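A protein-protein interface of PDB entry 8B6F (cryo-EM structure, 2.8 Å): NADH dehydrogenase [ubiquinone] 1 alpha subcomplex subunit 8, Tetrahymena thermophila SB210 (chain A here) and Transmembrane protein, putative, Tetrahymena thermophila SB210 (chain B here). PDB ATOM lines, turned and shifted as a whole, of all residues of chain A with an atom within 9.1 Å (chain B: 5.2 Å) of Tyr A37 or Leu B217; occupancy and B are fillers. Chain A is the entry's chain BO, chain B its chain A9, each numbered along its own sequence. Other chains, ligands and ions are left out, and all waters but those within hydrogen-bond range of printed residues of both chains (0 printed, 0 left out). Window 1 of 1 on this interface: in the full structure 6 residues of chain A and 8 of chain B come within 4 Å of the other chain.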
ATOM      1  N   LYS A  31     -29.546 -20.454  14.754  1.00  0.00           N
ATOM      2  CA  LYS A  31     -29.218 -21.430  13.719  1.00  0.00           C
ATOM      3  C   LYS A  31     -28.574 -20.764  12.510  1.00  0.00           C
ATOM      4  O   LYS A  31     -27.658 -21.329  11.903  1.00  0.00           O
ATOM      5  CB  LYS A  31     -30.471 -22.203  13.310  1.00  0.00           C
ATOM      6  CG  LYS A  31     -31.005 -23.131  14.394  1.00  0.00           C
ATOM      7  CD  LYS A  31     -29.988 -24.197  14.776  1.00  0.00           C
ATOM      8  CE  LYS A  31     -30.560 -25.172  15.789  1.00  0.00           C
ATOM      9  NZ  LYS A  31     -29.548 -26.177  16.216  1.00  0.00           N
ATOM     10  N   ASN A  32     -29.033 -19.567  12.141  1.00  0.00           N
ATOM     11  CA  ASN A  32     -28.385 -18.853  11.046  1.00  0.00           C
ATOM     12  C   ASN A  32     -26.944 -18.508  11.395  1.00  0.00           C
ATOM     13  O   ASN A  32     -26.044 -18.651  10.562  1.00  0.00           O
ATOM     14  CB  ASN A  32     -29.169 -17.585  10.702  1.00  0.00           C
ATOM     15  CG  ASN A  32     -30.420 -17.874   9.897  1.00  0.00           C
ATOM     16  OD1 ASN A  32     -30.451 -18.799   9.089  1.00  0.00           O
ATOM     17  ND2 ASN A  32     -31.457 -17.073  10.110  1.00  0.00           N
ATOM     18  N   LYS A  33     -26.707 -18.044  12.622  1.00  0.00           N
ATOM     19  CA  LYS A  33     -25.346 -17.712  13.025  1.00  0.00           C
ATOM     20  C   LYS A  33     -24.453 -18.946  13.013  1.00  0.00           C
ATOM     21  O   LYS A  33     -23.274 -18.866  12.652  1.00  0.00           O
ATOM     22  CB  LYS A  33     -25.359 -17.065  14.409  1.00  0.00           C
ATOM     23  CG  LYS A  33     -23.982 -16.745  14.961  1.00  0.00           C
ATOM     24  CD  LYS A  33     -24.033 -15.580  15.942  1.00  0.00           C
ATOM     25  CE  LYS A  33     -24.970 -15.854  17.112  1.00  0.00           C
ATOM     26  NZ  LYS A  33     -25.027 -14.696  18.050  1.00  0.00           N
ATOM     27  N   GLU A  34     -24.997 -20.097  13.414  1.00  0.00           N
ATOM     28  CA  GLU A  34     -24.202 -21.319  13.463  1.00  0.00           C
ATOM     29  C   GLU A  34     -23.979 -21.926  12.083  1.00  0.00           C
ATOM     30  O   GLU A  34     -22.914 -22.501  11.835  1.00  0.00           O
ATOM     31  CB  GLU A  34     -24.874 -22.344  14.374  1.00  0.00           C
ATOM     32  CG  GLU A  34     -24.906 -21.941  15.838  1.00  0.00           C
ATOM     33  CD  GLU A  34     -25.610 -22.963  16.705  1.00  0.00           C
ATOM     34  OE1 GLU A  34     -25.959 -24.042  16.186  1.00  0.00           O
ATOM     35  OE2 GLU A  34     -25.817 -22.685  17.905  1.00  0.00           O
ATOM     36  N   CYS A  35     -24.954 -21.816  11.183  1.00  0.00           N
ATOM     37  CA  CYS A  35     -24.917 -22.525   9.910  1.00  0.00           C
ATOM     38  C   CYS A  35     -24.678 -21.605   8.720  1.00  0.00           C
ATOM     39  O   CYS A  35     -24.828 -22.044   7.575  1.00  0.00           O
ATOM     40  CB  CYS A  35     -26.223 -23.296   9.702  1.00  0.00           C
ATOM     41  SG  CYS A  35     -26.881 -24.097  11.182  1.00  0.00           S
ATOM     42  N   GLY A  36     -24.312 -20.346   8.952  1.00  0.00           N
ATOM     43  CA  GLY A  36     -24.082 -19.437   7.842  1.00  0.00           C
ATOM     44  C   GLY A  36     -23.007 -19.900   6.885  1.00  0.00           C
ATOM     45  O   GLY A  36     -23.003 -19.486   5.722  1.00  0.00           O
ATOM     46  N   TYR A  37     -22.092 -20.752   7.346  1.00  0.00           N
ATOM     47  CA  TYR A  37     -21.059 -21.282   6.462  1.00  0.00           C
ATOM     48  C   TYR A  37     -21.671 -22.069   5.314  1.00  0.00           C
ATOM     49  O   TYR A  37     -21.215 -21.975   4.170  1.00  0.00           O
ATOM     50  CB  TYR A  37     -20.100 -22.155   7.270  1.00  0.00           C
ATOM     51  CG  TYR A  37     -19.036 -22.844   6.453  1.00  0.00           C
ATOM     52  CD1 TYR A  37     -17.878 -22.176   6.085  1.00  0.00           C
ATOM     53  CD2 TYR A  37     -19.178 -24.170   6.074  1.00  0.00           C
ATOM     54  CE1 TYR A  37     -16.898 -22.803   5.348  1.00  0.00           C
ATOM     55  CE2 TYR A  37     -18.203 -24.807   5.337  1.00  0.00           C
ATOM     56  CZ  TYR A  37     -17.064 -24.118   4.980  1.00  0.00           C
ATOM     57  OH  TYR A  37     -16.090 -24.745   4.246  1.00  0.00           O
ATOM     58  N   TYR A  38     -22.708 -22.857   5.602  1.00  0.00           N
ATOM     59  CA  TYR A  38     -23.317 -23.692   4.574  1.00  0.00           C
ATOM     60  C   TYR A  38     -23.977 -22.855   3.487  1.00  0.00           C
ATOM     61  O   TYR A  38     -23.939 -23.220   2.307  1.00  0.00           O
ATOM     62  CB  TYR A  38     -24.335 -24.634   5.213  1.00  0.00           C
ATOM     63  CG  TYR A  38     -23.723 -25.666   6.131  1.00  0.00           C
ATOM     64  CD1 TYR A  38     -22.574 -26.358   5.768  1.00  0.00           C
ATOM     65  CD2 TYR A  38     -24.292 -25.944   7.365  1.00  0.00           C
ATOM     66  CE1 TYR A  38     -22.014 -27.299   6.602  1.00  0.00           C
ATOM     67  CE2 TYR A  38     -23.739 -26.886   8.209  1.00  0.00           C
ATOM     68  CZ  TYR A  38     -22.599 -27.560   7.822  1.00  0.00           C
ATOM     69  OH  TYR A  38     -22.045 -28.497   8.660  1.00  0.00           O
ATOM     70  N   LEU A  39     -24.585 -21.727   3.859  1.00  0.00           N
ATOM     71  CA  LEU A  39     -25.255 -20.895   2.865  1.00  0.00           C
ATOM     72  C   LEU A  39     -24.248 -20.245   1.926  1.00  0.00           C
ATOM     73  O   LEU A  39     -24.450 -20.228   0.706  1.00  0.00           O
ATOM     74  CB  LEU A  39     -26.109 -19.835   3.559  1.00  0.00           C
ATOM     75  CG  LEU A  39     -27.125 -19.093   2.685  1.00  0.00           C
ATOM     76  CD1 LEU A  39     -28.170 -20.043   2.115  1.00  0.00           C
ATOM     77  CD2 LEU A  39     -27.789 -17.987   3.478  1.00  0.00           C
ATOM     78  N   GLN A  40     -23.159 -19.706   2.471  1.00  0.00           N
ATOM     79  CA  GLN A  40     -22.100 -19.175   1.622  1.00  0.00           C
ATOM     80  C   GLN A  40     -21.517 -20.274   0.746  1.00  0.00           C
ATOM     81  O   GLN A  40     -21.204 -20.045  -0.427  1.00  0.00           O
ATOM     82  CB  GLN A  40     -21.009 -18.534   2.478  1.00  0.00           C
ATOM     83  CG  GLN A  40     -20.020 -17.695   1.684  1.00  0.00           C
ATOM     84  CD  GLN A  40     -20.624 -16.409   1.162  1.00  0.00           C
ATOM     85  OE1 GLN A  40     -20.541 -16.110  -0.028  1.00  0.00           O
ATOM     86  NE2 GLN A  40     -21.233 -15.635   2.052  1.00  0.00           N
ATOM     87  N   GLY A  41     -21.369 -21.474   1.302  1.00  0.00           N
ATOM     88  CA  GLY A  41     -20.924 -22.601   0.502  1.00  0.00           C
ATOM     89  C   GLY A  41     -21.872 -22.918  -0.637  1.00  0.00           C
ATOM     90  O   GLY A  41     -21.440 -23.252  -1.742  1.00  0.00           O
ATOM     91  N   ILE A  42     -23.177 -22.832  -0.381  1.00  0.00           N
ATOM     92  CA  ILE A  42     -24.150 -23.086  -1.438  1.00  0.00           C
ATOM     93  C   ILE A  42     -23.988 -22.070  -2.559  1.00  0.00           C
ATOM     94  O   ILE A  42     -24.008 -22.425  -3.744  1.00  0.00           O
ATOM     95  CB  ILE A  42     -25.577 -23.072  -0.856  1.00  0.00           C
ATOM     96  CG1 ILE A  42     -25.806 -24.316   0.005  1.00  0.00           C
ATOM     97  CG2 ILE A  42     -26.618 -23.013  -1.970  1.00  0.00           C
ATOM     98  CD1 ILE A  42     -27.061 -24.256   0.850  1.00  0.00           C
ATOM     99  N   GLU A  43     -23.837 -20.791  -2.212  1.00  0.00           N
ATOM    100  CA  GLU A  43     -23.647 -19.771  -3.237  1.00  0.00           C
ATOM    101  C   GLU A  43     -22.390 -20.044  -4.050  1.00  0.00           C
ATOM    102  O   GLU A  43     -22.424 -20.062  -5.285  1.00  0.00           O
ATOM    103  CB  GLU A  43     -23.562 -18.389  -2.593  1.00  0.00           C
ATOM    104  CG  GLU A  43     -23.621 -17.252  -3.600  1.00  0.00           C
ATOM    105  CD  GLU A  43     -23.047 -15.956  -3.063  1.00  0.00           C
ATOM    106  OE1 GLU A  43     -22.278 -16.002  -2.082  1.00  0.00           O
ATOM    107  OE2 GLU A  43     -23.364 -14.887  -3.624  1.00  0.00           O
ATOM    108  N   GLN A  44     -21.261 -20.250  -3.367  1.00  0.00           N
ATOM    109  CA  GLN A  44     -19.998 -20.438  -4.068  1.00  0.00           C
ATOM    110  C   GLN A  44     -20.036 -21.690  -4.931  1.00  0.00           C
ATOM    111  O   GLN A  44     -19.547 -21.687  -6.067  1.00  0.00           O
ATOM    112  CB  GLN A  44     -18.849 -20.515  -3.063  1.00  0.00           C
ATOM    113  CG  GLN A  44     -18.684 -19.262  -2.217  1.00  0.00           C
ATOM    114  CD  GLN A  44     -18.299 -18.047  -3.031  1.00  0.00           C
ATOM    115  OE1 GLN A  44     -17.869 -18.162  -4.176  1.00  0.00           O
ATOM    116  NE2 GLN A  44     -18.459 -16.868  -2.443  1.00  0.00           N
ATOM    117  N   CYS A  45     -20.613 -22.773  -4.409  1.00  0.00           N
ATOM    118  CA  CYS A  45     -20.691 -24.010  -5.174  1.00  0.00           C
ATOM    119  C   CYS A  45     -21.655 -23.887  -6.345  1.00  0.00           C
ATOM    120  O   CYS A  45     -21.413 -24.474  -7.403  1.00  0.00           O
ATOM    121  CB  CYS A  45     -21.111 -25.165  -4.266  1.00  0.00           C
ATOM    122  SG  CYS A  45     -21.088 -26.777  -5.076  1.00  0.00           S
ATOM    123  N   LEU A  71     -24.255 -29.916   0.282  1.00  0.00           N
ATOM    124  CA  LEU A  71     -24.306 -28.656   1.015  1.00  0.00           C
ATOM    125  C   LEU A  71     -25.725 -28.334   1.466  1.00  0.00           C
ATOM    126  O   LEU A  71     -25.938 -27.903   2.605  1.00  0.00           O
ATOM    127  CB  LEU A  71     -23.756 -27.524   0.147  1.00  0.00           C
ATOM    128  CG  LEU A  71     -22.235 -27.460   0.022  1.00  0.00           C
ATOM    129  CD1 LEU A  71     -21.837 -26.548  -1.122  1.00  0.00           C
ATOM    130  CD2 LEU A  71     -21.614 -26.985   1.323  1.00  0.00           C
ATOM    131  N   ALA A  74     -26.655 -30.636   4.335  1.00  0.00           N
ATOM    132  CA  ALA A  74     -25.964 -30.235   5.554  1.00  0.00           C
ATOM    133  C   ALA A  74     -26.593 -28.987   6.153  1.00  0.00           C
ATOM    134  O   ALA A  74     -26.765 -28.895   7.374  1.00  0.00           O
ATOM    135  CB  ALA A  74     -24.484 -29.999   5.263  1.00  0.00           C
ATOM    136  N   HIS A  75     -26.945 -28.015   5.312  1.00  0.00           N
ATOM    137  CA  HIS A  75     -27.589 -26.810   5.817  1.00  0.00           C
ATOM    138  C   HIS A  75     -28.931 -27.138   6.452  1.00  0.00           C
ATOM    139  O   HIS A  75     -29.266 -26.612   7.519  1.00  0.00           O
ATOM    140  CB  HIS A  75     -27.761 -25.793   4.689  1.00  0.00           C
ATOM    141  CG  HIS A  75     -28.129 -24.423   5.164  1.00  0.00           C
ATOM    142  ND1 HIS A  75     -27.489 -23.804   6.216  1.00  0.00           N
ATOM    143  CD2 HIS A  75     -29.062 -23.548   4.726  1.00  0.00           C
ATOM    144  CE1 HIS A  75     -28.015 -22.609   6.409  1.00  0.00           C
ATOM    145  NE2 HIS A  75     -28.973 -22.428   5.517  1.00  0.00           N
ATOM    146  N   CYS A  78     -28.297 -28.773   9.815  1.00  0.00           N
ATOM    147  CA  CYS A  78     -27.824 -27.792  10.786  1.00  0.00           C
ATOM    148  C   CYS A  78     -28.960 -26.900  11.268  1.00  0.00           C
ATOM    149  O   CYS A  78     -29.068 -26.609  12.465  1.00  0.00           O
ATOM    150  CB  CYS A  78     -26.704 -26.954  10.169  1.00  0.00           C
ATOM    151  SG  CYS A  78     -25.858 -25.845  11.317  1.00  0.00           S
ATOM    152  N   MET A  79     -29.825 -26.461  10.352  1.00  0.00           N
ATOM    153  CA  MET A  79     -30.925 -25.583  10.737  1.00  0.00           C
ATOM    154  C   MET A  79     -31.953 -26.317  11.587  1.00  0.00           C
ATOM    155  O   MET A  79     -32.523 -25.735  12.517  1.00  0.00           O
ATOM    156  CB  MET A  79     -31.588 -24.997   9.491  1.00  0.00           C
ATOM    157  CG  MET A  79     -30.709 -24.038   8.704  1.00  0.00           C
ATOM    158  SD  MET A  79     -30.216 -22.581   9.642  1.00  0.00           S
ATOM    159  CE  MET A  79     -31.804 -21.820   9.973  1.00  0.00           C
ATOM    160  N   ARG A 117     -32.602 -17.304   0.679  1.00  0.00           N
ATOM    161  CA  ARG A 117     -32.545 -17.509   2.122  1.00  0.00           C
ATOM    162  C   ARG A 117     -33.895 -17.248   2.769  1.00  0.00           C
ATOM    163  O   ARG A 117     -34.220 -17.854   3.796  1.00  0.00           O
ATOM    164  CB  ARG A 117     -31.484 -16.609   2.756  1.00  0.00           C
ATOM    165  CG  ARG A 117     -31.697 -16.401   4.252  1.00  0.00           C
ATOM    166  CD  ARG A 117     -30.483 -15.801   4.930  1.00  0.00           C
ATOM    167  NE  ARG A 117     -30.737 -15.540   6.342  1.00  0.00           N
ATOM    168  CZ  ARG A 117     -29.810 -15.181   7.220  1.00  0.00           C
ATOM    169  NH1 ARG A 117     -28.542 -15.046   6.871  1.00  0.00           N
ATOM    170  NH2 ARG A 117     -30.166 -14.948   8.480  1.00  0.00           N
ATOM    171  N   ASP B 212     -19.151 -27.391  16.080  1.00  0.00           N
ATOM    172  CA  ASP B 212     -18.498 -26.208  16.628  1.00  0.00           C
ATOM    173  C   ASP B 212     -17.440 -25.676  15.675  1.00  0.00           C
ATOM    174  O   ASP B 212     -17.295 -24.460  15.512  1.00  0.00           O
ATOM    175  CB  ASP B 212     -17.878 -26.527  17.987  1.00  0.00           C
ATOM    176  CG  ASP B 212     -18.917 -26.745  19.064  1.00  0.00           C
ATOM    177  OD1 ASP B 212     -20.119 -26.578  18.773  1.00  0.00           O
ATOM    178  OD2 ASP B 212     -18.532 -27.081  20.203  1.00  0.00           O
ATOM    179  N   TYR B 213     -16.694 -26.573  15.031  1.00  0.00           N
ATOM    180  CA  TYR B 213     -15.707 -26.133  14.054  1.00  0.00           C
ATOM    181  C   TYR B 213     -16.371 -25.466  12.855  1.00  0.00           C
ATOM    182  O   TYR B 213     -15.873 -24.455  12.347  1.00  0.00           O
ATOM    183  CB  TYR B 213     -14.859 -27.317  13.591  1.00  0.00           C
ATOM    184  CG  TYR B 213     -13.929 -26.934  12.477  1.00  0.00           C
ATOM    185  CD1 TYR B 213     -12.835 -26.120  12.725  1.00  0.00           C
ATOM    186  CD2 TYR B 213     -14.151 -27.360  11.176  1.00  0.00           C
ATOM    187  CE1 TYR B 213     -11.982 -25.752  11.720  1.00  0.00           C
ATOM    188  CE2 TYR B 213     -13.300 -26.993  10.156  1.00  0.00           C
ATOM    189  CZ  TYR B 213     -12.219 -26.181  10.441  1.00  0.00           C
ATOM    190  OH  TYR B 213     -11.354 -25.802   9.452  1.00  0.00           O
ATOM    191  N   ILE B 214     -17.494 -26.012  12.387  1.00  0.00           N
ATOM    192  CA  ILE B 214     -18.205 -25.390  11.274  1.00  0.00           C
ATOM    193  C   ILE B 214     -18.649 -23.985  11.655  1.00  0.00           C
ATOM    194  O   ILE B 214     -18.545 -23.046  10.856  1.00  0.00           O
ATOM    195  CB  ILE B 214     -19.393 -26.269  10.840  1.00  0.00           C
ATOM    196  CG1 ILE B 214     -18.900 -27.587  10.231  1.00  0.00           C
ATOM    197  CG2 ILE B 214     -20.288 -25.529   9.849  1.00  0.00           C
ATOM    198  CD1 ILE B 214     -18.078 -27.441   8.963  1.00  0.00           C
ATOM    199  N   GLN B 215     -19.162 -23.815  12.875  1.00  0.00           N
ATOM    200  CA  GLN B 215     -19.520 -22.480  13.340  1.00  0.00           C
ATOM    201  C   GLN B 215     -18.289 -21.589  13.427  1.00  0.00           C
ATOM    202  O   GLN B 215     -18.330 -20.417  13.036  1.00  0.00           O
ATOM    203  CB  GLN B 215     -20.218 -22.558  14.697  1.00  0.00           C
ATOM    204  CG  GLN B 215     -20.596 -21.196  15.255  1.00  0.00           C
ATOM    205  CD  GLN B 215     -21.367 -21.288  16.551  1.00  0.00           C
ATOM    206  OE1 GLN B 215     -21.540 -22.369  17.111  1.00  0.00           O
ATOM    207  NE2 GLN B 215     -21.840 -20.146  17.037  1.00  0.00           N
ATOM    208  N   PHE B 216     -17.183 -22.131  13.943  1.00  0.00           N
ATOM    209  CA  PHE B 216     -15.961 -21.350  14.089  1.00  0.00           C
ATOM    210  C   PHE B 216     -15.449 -20.852  12.747  1.00  0.00           C
ATOM    211  O   PHE B 216     -14.871 -19.763  12.671  1.00  0.00           O
ATOM    212  CB  PHE B 216     -14.898 -22.197  14.791  1.00  0.00           C
ATOM    213  CG  PHE B 216     -13.492 -21.745  14.540  1.00  0.00           C
ATOM    214  CD1 PHE B 216     -12.939 -20.716  15.282  1.00  0.00           C
ATOM    215  CD2 PHE B 216     -12.713 -22.366  13.578  1.00  0.00           C
ATOM    216  CE1 PHE B 216     -11.640 -20.304  15.058  1.00  0.00           C
ATOM    217  CE2 PHE B 216     -11.416 -21.960  13.351  1.00  0.00           C
ATOM    218  CZ  PHE B 216     -10.878 -20.927  14.092  1.00  0.00           C
ATOM    219  N   LEU B 217     -15.646 -21.630  11.680  1.00  0.00           N
ATOM    220  CA  LEU B 217     -15.214 -21.192  10.357  1.00  0.00           C
ATOM    221  C   LEU B 217     -15.773 -19.817  10.022  1.00  0.00           C
ATOM    222  O   LEU B 217     -15.085 -18.991   9.414  1.00  0.00           O
ATOM    223  CB  LEU B 217     -15.639 -22.214   9.301  1.00  0.00           C
ATOM    224  CG  LEU B 217     -14.809 -23.498   9.226  1.00  0.00           C
ATOM    225  CD1 LEU B 217     -15.435 -24.476   8.255  1.00  0.00           C
ATOM    226  CD2 LEU B 217     -13.375 -23.203   8.820  1.00  0.00           C
ATOM    227  N   GLY B 218     -17.006 -19.540  10.439  1.00  0.00           N
ATOM    228  CA  GLY B 218     -17.616 -18.255  10.149  1.00  0.00           C
ATOM    229  C   GLY B 218     -16.872 -17.077  10.740  1.00  0.00           C
ATOM    230  O   GLY B 218     -17.096 -15.939  10.316  1.00  0.00           O
ATOM    231  N   ASN B 219     -15.994 -17.318  11.716  1.00  0.00           N
ATOM    232  CA  ASN B 219     -15.217 -16.225  12.290  1.00  0.00           C
ATOM    233  C   ASN B 219     -14.311 -15.585  11.246  1.00  0.00           C
ATOM    234  O   ASN B 219     -14.159 -14.359  11.216  1.00  0.00           O
ATOM    235  CB  ASN B 219     -14.394 -16.729  13.473  1.00  0.00           C
ATOM    236  CG  ASN B 219     -15.245 -17.031  14.687  1.00  0.00           C
ATOM    237  OD1 ASN B 219     -16.470 -17.097  14.600  1.00  0.00           O
ATOM    238  ND2 ASN B 219     -14.598 -17.217  15.831  1.00  0.00           N
ATOM    239  N   TYR B 220     -13.696 -16.397  10.389  1.00  0.00           N
ATOM    240  CA  TYR B 220     -12.829 -15.862   9.348  1.00  0.00           C
ATOM    241  C   TYR B 220     -13.604 -14.907   8.450  1.00  0.00           C
ATOM    242  O   TYR B 220     -14.721 -15.206   8.020  1.00  0.00           O
ATOM    243  CB  TYR B 220     -12.235 -17.004   8.524  1.00  0.00           C
ATOM    244  CG  TYR B 220     -11.263 -17.851   9.300  1.00  0.00           C
ATOM    245  CD1 TYR B 220      -9.988 -17.390   9.584  1.00  0.00           C
ATOM    246  CD2 TYR B 220     -11.621 -19.112   9.752  1.00  0.00           C
ATOM    247  CE1 TYR B 220      -9.097 -18.158  10.296  1.00  0.00           C
ATOM    248  CE2 TYR B 220     -10.737 -19.887  10.465  1.00  0.00           C
ATOM    249  CZ  TYR B 220      -9.479 -19.402  10.740  1.00  0.00           C
ATOM    250  OH  TYR B 220      -8.594 -20.174  11.449  1.00  0.00           O
ATOM    251  N   VAL B 223     -14.098 -16.210   4.515  1.00  0.00           N
ATOM    252  CA  VAL B 223     -15.145 -17.199   4.280  1.00  0.00           C
ATOM    253  C   VAL B 223     -16.521 -16.581   4.494  1.00  0.00           C
ATOM    254  O   VAL B 223     -17.459 -16.847   3.732  1.00  0.00           O
ATOM    255  CB  VAL B 223     -14.937 -18.436   5.175  1.00  0.00           C
ATOM    256  CG1 VAL B 223     -13.555 -19.024   4.975  1.00  0.00           C
ATOM    257  CG2 VAL B 223     -15.169 -18.105   6.628  1.00  0.00           C
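Of the 21 printed residues of chain A, 4 touch a printed residue of chain B.
Printed residues of chain A that touch a printed residue of chain B: Glu A34, Tyr A37, Tyr A38 and Gln A40.
Of the 10 printed residues of chain B, 4 touch a printed residue of chain A.
Hydrophobic or aromatic side chains of chain B within 4 Å of the printed part of chain A: Ile B214 and Leu B217.
Among the printed residues, no Asp or Glu carboxylate lies within 4 Å of a Lys or Arg side-chain nitrogen of the other chain.
The side-chain carboxylate of Glu A43 sits close to the side-chain amide oxygen of Gln A40, 2.7 Å away.
OE1 of Gln A40 sits at hydrogen-bond distance from NE2 of Gln A44, at 3.3 Å.
SG of Cys A35 forms a disulfide with SG of Cys A78, at 2.0 Å.
Among the printed residues, pairs that only touch across the chains: Gln A40 with Val B223 (3.4 Å), Glu A34 with Gln B215 (3.6 Å), Tyr A38 with Ile B214 (3.6 Å) and Tyr A37 with Leu B217 (3.7 Å).
Of the printed residues of chain B, Tyr A37 touches Leu B217.
Leu B217 touches just one residue of chain A: Tyr A37 (3.7 Å).
Of the printed residues of chain A, Ile B214 touches Tyr A38 (3.6 Å).
Of the printed residues of chain B, Tyr A38 touches Ile B214.
Leu A71 touches none of the printed residues of chain B.
Gly A41 touches none of the printed residues of chain B.
The nearest printed residue of chain A that does not touch Leu B217 is Glu A34 (7.3 Å).
The nearest printed residue of chain B that does not touch Gln A40 is Gly B218 (8.4 Å).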
